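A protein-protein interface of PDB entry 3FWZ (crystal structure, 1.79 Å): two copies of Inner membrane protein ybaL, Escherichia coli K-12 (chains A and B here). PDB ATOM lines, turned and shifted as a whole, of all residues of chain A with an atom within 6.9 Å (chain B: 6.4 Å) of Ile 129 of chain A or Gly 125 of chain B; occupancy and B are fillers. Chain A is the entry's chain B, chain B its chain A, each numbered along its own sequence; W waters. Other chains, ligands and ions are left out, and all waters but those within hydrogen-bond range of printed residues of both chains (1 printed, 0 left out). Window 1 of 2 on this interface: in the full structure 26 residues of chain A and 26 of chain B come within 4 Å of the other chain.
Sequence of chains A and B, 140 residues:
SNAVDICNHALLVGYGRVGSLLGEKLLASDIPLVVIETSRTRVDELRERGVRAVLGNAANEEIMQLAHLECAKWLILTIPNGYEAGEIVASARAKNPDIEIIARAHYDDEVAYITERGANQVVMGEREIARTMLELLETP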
ATOM      1  N   VAL A  18      -7.091  11.298  14.957  1.00  0.00           N
ATOM      2  CA  VAL A  18      -8.486  11.255  15.444  1.00  0.00           C
ATOM      3  C   VAL A  18      -9.327  10.366  14.554  1.00  0.00           C
ATOM      4  O   VAL A  18     -10.021   9.467  15.050  1.00  0.00           O
ATOM      5  CB  VAL A  18      -9.079  12.688  15.496  1.00  0.00           C
ATOM      6  CG1 VAL A  18     -10.562  12.654  15.926  1.00  0.00           C
ATOM      7  CG2 VAL A  18      -8.276  13.548  16.505  1.00  0.00           C
ATOM      8  N   HIS A 106     -10.268  23.152  18.686  1.00  0.00           N
ATOM      9  CA  HIS A 106      -9.184  23.278  19.639  1.00  0.00           C
ATOM     10  C   HIS A 106      -9.234  24.615  20.400  1.00  0.00           C
ATOM     11  O   HIS A 106      -8.430  24.835  21.298  1.00  0.00           O
ATOM     12  CB  HIS A 106      -7.817  23.087  18.953  1.00  0.00           C
ATOM     13  CG  HIS A 106      -7.624  21.679  18.479  1.00  0.00           C
ATOM     14  ND1 HIS A 106      -7.308  20.658  19.352  1.00  0.00           N
ATOM     15  CD2 HIS A 106      -7.849  21.098  17.275  1.00  0.00           C
ATOM     16  CE1 HIS A 106      -7.274  19.512  18.684  1.00  0.00           C
ATOM     17  NE2 HIS A 106      -7.616  19.746  17.429  1.00  0.00           N
ATOM     18  N   MET A 124     -14.056  19.681  21.625  1.00  0.00           N
ATOM     19  CA  MET A 124     -12.843  20.493  21.729  1.00  0.00           C
ATOM     20  C   MET A 124     -11.804  19.700  22.469  1.00  0.00           C
ATOM     21  O   MET A 124     -11.991  19.334  23.621  1.00  0.00           O
ATOM     22  CB  MET A 124     -13.121  21.847  22.410  1.00  0.00           C
ATOM     23  CG  MET A 124     -11.855  22.695  22.579  1.00  0.00           C
ATOM     24  SD  MET A 124     -12.354  24.442  23.280  1.00  0.00           S
ATOM     25  CE  MET A 124     -10.572  24.936  23.990  1.00  0.00           C
ATOM     26  N   GLY A 125     -10.679  19.439  21.806  1.00  0.00           N
ATOM     27  CA  GLY A 125      -9.673  18.548  22.379  1.00  0.00           C
ATOM     28  C   GLY A 125      -9.219  19.004  23.735  1.00  0.00           C
ATOM     29  O   GLY A 125      -9.150  18.209  24.686  1.00  0.00           O
ATOM     30  N   GLU A 126      -8.904  20.297  23.846  1.00  0.00           N
ATOM     31  CA  GLU A 126      -8.335  20.767  25.105  1.00  0.00           C
ATOM     32  C   GLU A 126      -9.338  20.701  26.256  1.00  0.00           C
ATOM     33  O   GLU A 126      -8.955  20.478  27.431  1.00  0.00           O
ATOM     34  CB  GLU A 126      -7.704  22.151  24.898  1.00  0.00           C
ATOM     35  CG  GLU A 126      -6.312  22.052  24.239  1.00  0.00           C
ATOM     36  CD  GLU A 126      -6.282  21.404  22.864  1.00  0.00           C
ATOM     37  OE1 GLU A 126      -7.222  21.563  22.066  1.00  0.00           O
ATOM     38  OE2 GLU A 126      -5.248  20.789  22.539  1.00  0.00           O
ATOM     39  N   ARG A 127     -10.627  20.858  25.950  1.00  0.00           N
ATOM     40  CA  ARG A 127     -11.659  20.690  26.976  1.00  0.00           C
ATOM     41  C   ARG A 127     -11.685  19.241  27.462  1.00  0.00           C
ATOM     42  O   ARG A 127     -11.864  18.982  28.676  1.00  0.00           O
ATOM     43  CB  ARG A 127     -13.037  21.058  26.390  1.00  0.00           C
ATOM     44  CG  ARG A 127     -14.093  21.500  27.390  1.00  0.00           C
ATOM     45  CD  ARG A 127     -15.275  22.154  26.634  1.00  0.00           C
ATOM     46  NE  ARG A 127     -15.020  23.536  26.189  1.00  0.00           N
ATOM     47  CZ  ARG A 127     -15.796  24.221  25.337  1.00  0.00           C
ATOM     48  NH1 ARG A 127     -16.879  23.667  24.791  1.00  0.00           N
ATOM     49  NH2 ARG A 127     -15.500  25.472  25.014  1.00  0.00           N
ATOM     50  N   GLU A 128     -11.547  18.302  26.517  1.00  0.00           N
ATOM     51  CA  GLU A 128     -11.623  16.881  26.855  1.00  0.00           C
ATOM     52  C   GLU A 128     -10.367  16.430  27.583  1.00  0.00           C
ATOM     53  O   GLU A 128     -10.453  15.578  28.450  1.00  0.00           O
ATOM     54  CB  GLU A 128     -11.916  15.992  25.643  1.00  0.00           C
ATOM     55  CG  GLU A 128     -13.227  16.376  24.941  1.00  0.00           C
ATOM     56  CD  GLU A 128     -14.413  16.310  25.880  1.00  0.00           C
ATOM     57  OE1 GLU A 128     -14.393  15.522  26.859  1.00  0.00           O
ATOM     58  OE2 GLU A 128     -15.350  17.068  25.649  1.00  0.00           O
ATOM     59  N   ILE A 129      -9.231  17.068  27.313  1.00  0.00           N
ATOM     60  CA  ILE A 129      -8.037  16.784  28.120  1.00  0.00           C
ATOM     61  C   ILE A 129      -8.302  17.174  29.578  1.00  0.00           C
ATOM     62  O   ILE A 129      -8.042  16.373  30.497  1.00  0.00           O
ATOM     63  CB  ILE A 129      -6.794  17.533  27.593  1.00  0.00           C
ATOM     64  CG1 ILE A 129      -6.417  17.052  26.184  1.00  0.00           C
ATOM     65  CG2 ILE A 129      -5.603  17.341  28.562  1.00  0.00           C
ATOM     66  CD1 ILE A 129      -5.384  18.016  25.460  1.00  0.00           C
ATOM     67  N   ALA A 130      -8.805  18.394  29.798  1.00  0.00           N
ATOM     68  CA  ALA A 130      -9.094  18.854  31.170  1.00  0.00           C
ATOM     69  C   ALA A 130     -10.113  17.924  31.820  1.00  0.00           C
ATOM     70  O   ALA A 130      -9.933  17.558  32.985  1.00  0.00           O
ATOM     71  CB  ALA A 130      -9.621  20.269  31.170  1.00  0.00           C
ATOM     72  N   ARG A 131     -11.147  17.529  31.071  1.00  0.00           N
ATOM     73  CA  ARG A 131     -12.198  16.663  31.663  1.00  0.00           C
ATOM     74  C   ARG A 131     -11.564  15.339  32.140  1.00  0.00           C
ATOM     75  O   ARG A 131     -11.836  14.827  33.256  1.00  0.00           O
ATOM     76  CB  ARG A 131     -13.313  16.361  30.658  1.00  0.00           C
ATOM     77  CG  ARG A 131     -14.580  15.743  31.340  1.00  0.00           C
ATOM     78  CD  ARG A 131     -15.634  15.368  30.307  1.00  0.00           C
ATOM     79  NE  ARG A 131     -15.748  16.347  29.207  1.00  0.00           N
ATOM     80  CZ  ARG A 131     -16.433  17.491  29.264  1.00  0.00           C
ATOM     81  NH1 ARG A 131     -16.455  18.291  28.198  1.00  0.00           N
ATOM     82  NH2 ARG A 131     -17.081  17.854  30.380  1.00  0.00           N
ATOM     83  N   THR A 132     -10.742  14.776  31.275  1.00  0.00           N
ATOM     84  CA  THR A 132     -10.132  13.494  31.585  1.00  0.00           C
ATOM     85  C   THR A 132      -9.173  13.603  32.751  1.00  0.00           C
ATOM     86  O   THR A 132      -9.142  12.721  33.618  1.00  0.00           O
ATOM     87  CB  THR A 132      -9.432  12.905  30.351  1.00  0.00           C
ATOM     88  OG1 THR A 132     -10.429  12.673  29.358  1.00  0.00           O
ATOM     89  CG2 THR A 132      -8.771  11.576  30.690  1.00  0.00           C
ATOM     90  N   MET A 133      -8.401  14.681  32.811  1.00  0.00           N
ATOM     91  CA  MET A 133      -7.470  14.848  33.936  1.00  0.00           C
ATOM     92  C   MET A 133      -8.244  14.979  35.251  1.00  0.00           C
ATOM     93  O   MET A 133      -7.831  14.430  36.270  1.00  0.00           O
ATOM     94  CB  MET A 133      -6.605  16.078  33.734  1.00  0.00           C
ATOM     95  CG  MET A 133      -5.552  15.899  32.637  1.00  0.00           C
ATOM     96  SD  MET A 133      -4.476  17.507  32.523  1.00  0.00           S
ATOM     97  CE  MET A 133      -3.067  16.756  31.390  1.00  0.00           C
ATOM     98  N   LEU A 134      -9.373  15.690  35.211  1.00  0.00           N
ATOM     99  CA  LEU A 134     -10.155  15.901  36.418  1.00  0.00           C
ATOM    100  C   LEU A 134     -10.707  14.582  36.920  1.00  0.00           C
ATOM    101  O   LEU A 134     -10.711  14.331  38.136  1.00  0.00           O
ATOM    102  CB  LEU A 134     -11.273  16.909  36.169  1.00  0.00           C
ATOM    103  CG  LEU A 134     -10.772  18.358  36.145  1.00  0.00           C
ATOM    104  CD1 LEU A 134     -11.853  19.244  35.495  1.00  0.00           C
ATOM    105  CD2 LEU A 134     -10.406  18.856  37.548  1.00  0.00           C
ATOM    106  N   GLU A 135     -11.141  13.737  35.986  1.00  0.00           N
ATOM    107  CA  GLU A 135     -11.592  12.386  36.322  1.00  0.00           C
ATOM    108  C   GLU A 135     -10.471  11.585  36.998  1.00  0.00           C
ATOM    109  O   GLU A 135     -10.725  10.841  37.927  1.00  0.00           O
ATOM    110  CB  GLU A 135     -12.137  11.650  35.082  1.00  0.00           C
ATOM    111  CG  GLU A 135     -13.440  12.260  34.533  1.00  0.00           C
ATOM    112  CD  GLU A 135     -13.723  11.915  33.049  1.00  0.00           C
ATOM    113  OE1 GLU A 135     -12.955  11.131  32.418  1.00  0.00           O
ATOM    114  OE2 GLU A 135     -14.719  12.449  32.507  1.00  0.00           O
ATOM    115  N   VAL B  18      -6.380  24.352  28.729  1.00  0.00           N
ATOM    116  CA  VAL B  18      -6.487  23.129  29.552  1.00  0.00           C
ATOM    117  C   VAL B  18      -6.407  23.479  31.034  1.00  0.00           C
ATOM    118  O   VAL B  18      -7.285  23.108  31.818  1.00  0.00           O
ATOM    119  CB  VAL B  18      -5.376  22.117  29.208  1.00  0.00           C
ATOM    120  CG1 VAL B  18      -5.520  20.847  30.084  1.00  0.00           C
ATOM    121  CG2 VAL B  18      -5.403  21.764  27.696  1.00  0.00           C
ATOM    122  N   LEU B  22      -8.991  23.013  34.569  1.00  0.00           N
ATOM    123  CA  LEU B  22      -8.581  22.269  35.765  1.00  0.00           C
ATOM    124  C   LEU B  22      -8.567  23.111  37.007  1.00  0.00           C
ATOM    125  O   LEU B  22      -9.072  22.695  38.060  1.00  0.00           O
ATOM    126  CB  LEU B  22      -7.188  21.699  35.599  1.00  0.00           C
ATOM    127  CG  LEU B  22      -7.263  20.258  35.157  1.00  0.00           C
ATOM    128  CD1 LEU B  22      -7.228  20.255  33.671  1.00  0.00           C
ATOM    129  CD2 LEU B  22      -6.100  19.502  35.675  1.00  0.00           C
ATOM    130  N   THR B  78       0.042  20.848  31.956  1.00  0.00           N
ATOM    131  CA  THR B  78      -0.943  21.105  30.914  1.00  0.00           C
ATOM    132  C   THR B  78      -0.352  21.838  29.706  1.00  0.00           C
ATOM    133  O   THR B  78      -1.085  22.387  28.882  1.00  0.00           O
ATOM    134  CB  THR B  78      -2.183  21.878  31.453  1.00  0.00           C
ATOM    135  OG1 THR B  78      -1.845  23.264  31.691  1.00  0.00           O
ATOM    136  CG2 THR B  78      -2.710  21.220  32.722  1.00  0.00           C
ATOM    137  N   ALA B 103       0.167  14.368  32.822  1.00  0.00           N
ATOM    138  CA  ALA B 103       0.653  15.240  31.748  1.00  0.00           C
ATOM    139  C   ALA B 103      -0.181  15.145  30.487  1.00  0.00           C
ATOM    140  O   ALA B 103      -0.842  14.126  30.227  1.00  0.00           O
ATOM    141  CB  ALA B 103       2.156  14.917  31.407  1.00  0.00           C
ATOM    142  N   ARG B 104      -0.138  16.230  29.716  1.00  0.00           N
ATOM    143  CA  ARG B 104      -0.797  16.330  28.421  1.00  0.00           C
ATOM    144  C   ARG B 104       0.146  15.929  27.265  1.00  0.00           C
ATOM    145  O   ARG B 104       1.359  16.161  27.316  1.00  0.00           O
ATOM    146  CB  ARG B 104      -1.247  17.779  28.246  1.00  0.00           C
ATOM    147  CG  ARG B 104      -1.659  18.208  26.829  1.00  0.00           C
ATOM    148  CD  ARG B 104      -1.976  19.731  26.885  1.00  0.00           C
ATOM    149  NE  ARG B 104      -2.385  20.261  25.562  1.00  0.00           N
ATOM    150  CZ  ARG B 104      -2.496  21.558  25.305  1.00  0.00           C
ATOM    151  NH1 ARG B 104      -2.204  22.441  26.252  1.00  0.00           N
ATOM    152  NH2 ARG B 104      -2.877  21.982  24.090  1.00  0.00           N
ATOM    153  N   ALA B 105      -0.416  15.344  26.216  1.00  0.00           N
ATOM    154  CA  ALA B 105       0.356  15.058  25.015  1.00  0.00           C
ATOM    155  C   ALA B 105      -0.554  15.060  23.800  1.00  0.00           C
ATOM    156  O   ALA B 105      -1.774  15.084  23.930  1.00  0.00           O
ATOM    157  CB  ALA B 105       1.061  13.671  25.130  1.00  0.00           C
ATOM    158  N   HIS B 106       0.057  14.991  22.613  1.00  0.00           N
ATOM    159  CA  HIS B 106      -0.711  15.014  21.366  1.00  0.00           C
ATOM    160  C   HIS B 106      -0.304  13.962  20.365  1.00  0.00           C
ATOM    161  O   HIS B 106      -0.984  13.756  19.371  1.00  0.00           O
ATOM    162  CB  HIS B 106      -0.661  16.421  20.774  1.00  0.00           C
ATOM    163  CG  HIS B 106      -1.391  17.399  21.633  1.00  0.00           C
ATOM    164  ND1 HIS B 106      -2.766  17.482  21.630  1.00  0.00           N
ATOM    165  CD2 HIS B 106      -0.957  18.224  22.618  1.00  0.00           C
ATOM    166  CE1 HIS B 106      -3.152  18.346  22.559  1.00  0.00           C
ATOM    167  NE2 HIS B 106      -2.069  18.828  23.154  1.00  0.00           N
ATOM    168  N   VAL B 123      -2.414  12.110  29.203  1.00  0.00           N
ATOM    169  CA  VAL B 123      -3.714  12.317  28.551  1.00  0.00           C
ATOM    170  C   VAL B 123      -3.436  12.909  27.167  1.00  0.00           C
ATOM    171  O   VAL B 123      -2.947  14.054  27.049  1.00  0.00           O
ATOM    172  CB  VAL B 123      -4.654  13.248  29.364  1.00  0.00           C
ATOM    173  CG1 VAL B 123      -5.991  13.407  28.659  1.00  0.00           C
ATOM    174  CG2 VAL B 123      -4.917  12.659  30.782  1.00  0.00           C
ATOM    175  N   MET B 124      -3.778  12.154  26.132  1.00  0.00           N
ATOM    176  CA  MET B 124      -3.489  12.575  24.731  1.00  0.00           C
ATOM    177  C   MET B 124      -4.743  13.154  24.114  1.00  0.00           C
ATOM    178  O   MET B 124      -5.763  12.470  24.020  1.00  0.00           O
ATOM    179  CB  MET B 124      -2.983  11.384  23.887  1.00  0.00           C
ATOM    180  CG  MET B 124      -2.554  11.817  22.457  1.00  0.00           C
ATOM    181  SD  MET B 124      -1.699  10.340  21.535  1.00  0.00           S
ATOM    182  CE  MET B 124      -2.466  10.617  19.765  1.00  0.00           C
ATOM    183  N   GLY B 125      -4.691  14.430  23.743  1.00  0.00           N
ATOM    184  CA  GLY B 125      -5.912  15.145  23.335  1.00  0.00           C
ATOM    185  C   GLY B 125      -6.642  14.414  22.224  1.00  0.00           C
ATOM    186  O   GLY B 125      -7.860  14.275  22.258  1.00  0.00           O
ATOM    187  N   GLU B 126      -5.894  13.941  21.238  1.00  0.00           N
ATOM    188  CA  GLU B 126      -6.538  13.400  20.033  1.00  0.00           C
ATOM    189  C   GLU B 126      -7.218  12.068  20.336  1.00  0.00           C
ATOM    190  O   GLU B 126      -8.253  11.755  19.744  1.00  0.00           O
ATOM    191  CB  GLU B 126      -5.549  13.379  18.846  1.00  0.00           C
ATOM    192  CG  GLU B 126      -5.434  14.760  18.182  1.00  0.00           C
ATOM    193  CD  GLU B 126      -4.879  15.860  19.105  1.00  0.00           C
ATOM    194  OE1 GLU B 126      -4.051  15.583  20.013  1.00  0.00           O
ATOM    195  OE2 GLU B 126      -5.257  17.036  18.879  1.00  0.00           O
ATOM    196  N   ARG B 127      -6.689  11.312  21.297  1.00  0.00           N
ATOM    197  CA  ARG B 127      -7.361  10.096  21.729  1.00  0.00           C
ATOM    198  C   ARG B 127      -8.666  10.410  22.451  1.00  0.00           C
ATOM    199  O   ARG B 127      -9.670   9.710  22.269  1.00  0.00           O
ATOM    200  CB  ARG B 127      -6.443   9.211  22.588  1.00  0.00           C
ATOM    201  CG  ARG B 127      -5.324   8.608  21.759  1.00  0.00           C
ATOM    202  CD  ARG B 127      -4.513   7.585  22.539  1.00  0.00           C
ATOM    203  NE  ARG B 127      -3.470   7.001  21.707  1.00  0.00           N
ATOM    204  CZ  ARG B 127      -3.632   5.904  20.965  1.00  0.00           C
ATOM    205  NH1 ARG B 127      -4.798   5.282  20.954  1.00  0.00           N
ATOM    206  NH2 ARG B 127      -2.628   5.438  20.234  1.00  0.00           N
ATOM    207  N   GLU B 128      -8.652  11.464  23.266  1.00  0.00           N
ATOM    208  CA  GLU B 128      -9.861  11.874  23.969  1.00  0.00           C
ATOM    209  C   GLU B 128     -10.880  12.445  22.994  1.00  0.00           C
ATOM    210  O   GLU B 128     -12.076  12.253  23.198  1.00  0.00           O
ATOM    211  CB  GLU B 128      -9.564  12.844  25.108  1.00  0.00           C
ATOM    212  CG  GLU B 128      -8.564  12.303  26.157  1.00  0.00           C
ATOM    213  CD  GLU B 128      -8.925  10.918  26.665  1.00  0.00           C
ATOM    214  OE1 GLU B 128     -10.123  10.662  26.946  1.00  0.00           O
ATOM    215  OE2 GLU B 128      -8.014  10.071  26.770  1.00  0.00           O
ATOM    216  N   ILE B 129     -10.428  13.140  21.942  1.00  0.00           N
ATOM    217  CA  ILE B 129     -11.392  13.585  20.903  1.00  0.00           C
ATOM    218  C   ILE B 129     -12.130  12.412  20.275  1.00  0.00           C
ATOM    219  O   ILE B 129     -13.370  12.399  20.183  1.00  0.00           O
ATOM    220  CB  ILE B 129     -10.734  14.407  19.797  1.00  0.00           C
ATOM    221  CG1 ILE B 129     -10.214  15.712  20.404  1.00  0.00           C
ATOM    222  CG2 ILE B 129     -11.826  14.811  18.759  1.00  0.00           C
ATOM    223  CD1 ILE B 129      -9.238  16.481  19.480  1.00  0.00           C
ATOM    224  N   ALA B 130     -11.381  11.389  19.876  1.00  0.00           N
ATOM    225  CA  ALA B 130     -11.977  10.211  19.216  1.00  0.00           C
ATOM    226  C   ALA B 130     -12.927   9.501  20.176  1.00  0.00           C
ATOM    227  O   ALA B 130     -14.063   9.131  19.810  1.00  0.00           O
ATOM    228  CB  ALA B 130     -10.863   9.260  18.725  1.00  0.00           C
HETATM  229  O   HOH W   1      -6.315  18.063  21.471  1.00  0.00           O
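Printed residues of chain B that touch a printed residue of chain A: Val 18, Leu 22, Ala 103, Arg 104, His 106, Val 123, Gly 125, Glu 126, Glu 128, Ile 129 and Ala 130. Hydrophobic or aromatic side chains of chain B within 4 Å of the printed part of chain A: Val 18, Leu 22, His 106, Val 123, Ile 129 and Ala 130. Hydrophobic or aromatic side chains of chain A within 4 Å of the printed part of chain B: Val 18, His 106, Ile 129, Ala 130 and Met 133. Among the printed residues, Asp or Glu carboxylates within 4 Å of a Lys or Arg side-chain nitrogen of the other chain: Glu 126 of chain A with Arg 104 of chain B.
ND1 of His 106 of chain A sits at hydrogen-bond distance from OE1 of Glu 126 of chain A. The side-chain hydroxyl of Thr 132 of chain A is in hydrogen-bond range of the backbone carbonyl oxygen of Glu 128 of chain A (3.0 Å). O of Ala 105 of chain B lies within hydrogen-bond range of N of Gly 125 of chain B (3.0 Å). N of Ala 105 of chain B lies within hydrogen-bond range of O of Val 123 of chain B (3.0 Å). OE1 of Glu 126 of chain B lies within hydrogen-bond range of ND1 of His 106 of chain B (2.8 Å). The side-chain carboxylate of Glu 128 of chain A lies within salt-bridge range of the guanidinium group of Arg 131 of chain A, at 2.8 Å.
The guanidinium group (NH2) of Arg 104 of chain B lies within salt-bridge range of the side-chain carboxylate (OE2) of Glu 126 of chain A (3.1 Å). The side-chain hydroxyl of Thr 132 of chain A is in hydrogen-bond range of the side-chain carboxylate of Glu 128 of chain B.
Val 18 of chain A touches Glu 126 of chain B, and with the chains exchanged Glu 126 of chain A touches Val 18 of chain B. Val 18 of chain A touches Ile 129 of chain B, and with the chains exchanged Ile 129 of chain A touches Val 18 of chain B. His 106 of chain A touches Glu 126 of chain B, and with the chains exchanged Glu 126 of chain A touches His 106 of chain B. Gly 125 of chain A touches Ile 129 of chain B, and with the chains exchanged Ile 129 of chain A touches Gly 125 of chain B. Positions printed for both chains: 18, 106, 124, 125, 126, 127, 128, 129 and 130.
Among the printed residues, pairs that only touch across the chains: Val 18 of chain A with Glu 126 of chain B (3.5 Å), Val 18 of chain A with Ile 129 of chain B (3.8 Å), Val 18 of chain A with Ala 130 of chain B (3.8 Å), His 106 of chain A with Glu 126 of chain B (3.2 Å), His 106 of chain A with Ile 129 of chain B (3.7 Å), Gly 125 of chain A with Ile 129 of chain B (3.5 Å), Glu 126 of chain A with Val 18 of chain B (3.6 Å), Glu 126 of chain A with His 106 of chain B (3.2 Å), Glu 128 of chain A with Glu 128 of chain B (3.97 Å), Ile 129 of chain A with Val 18 of chain B (3.8 Å), Ile 129 of chain A with Arg 104 of chain B (3.7 Å), Ile 129 of chain A with His 106 of chain B (3.7 Å), Ile 129 of chain A with Val 123 of chain B (3.95 Å), Ile 129 of chain A with Gly 125 of chain B (3.5 Å), Ala 130 of chain A with Val 18 of chain B (3.7 Å), Ala 130 of chain A with Leu 22 of chain B (3.4 Å), Thr 132 of chain A with Val 123 of chain B (3.9 Å), Met 133 of chain A with Leu 22 of chain B (3.97 Å), Met 133 of chain A with Ala 103 of chain B (3.4 Å), Met 133 of chain A with Arg 104 of chain B (3.4 Å) and Met 133 of chain A with Val 123 of chain B (3.8 Å).
Water W1 lies within hydrogen-bond range of OE2 of Glu 126 of chain B (3.0 Å), OE2 of Glu 126 of chain A (3.1 Å) and ND1 of His 106 of chain A (3.5 Å).
Printed residues of chain A within 4 Å of Val 123 of chain B: Ile 129 (3.95 Å), Thr 132 (3.9 Å) and Met 133 (3.8 Å). Gly 125 of chain B touches just one residue of chain A: Ile 129. Of the printed residues of chain A, Glu 128 of chain B touches Glu 128 and Thr 132. The nearest residue of chain B that does not touch Ile 129 of chain A is Met 124 of chain B (4.7 Å). The nearest residue of chain A that does not touch Gly 125 of chain B is Gly 125 of chain A (4.6 Å).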
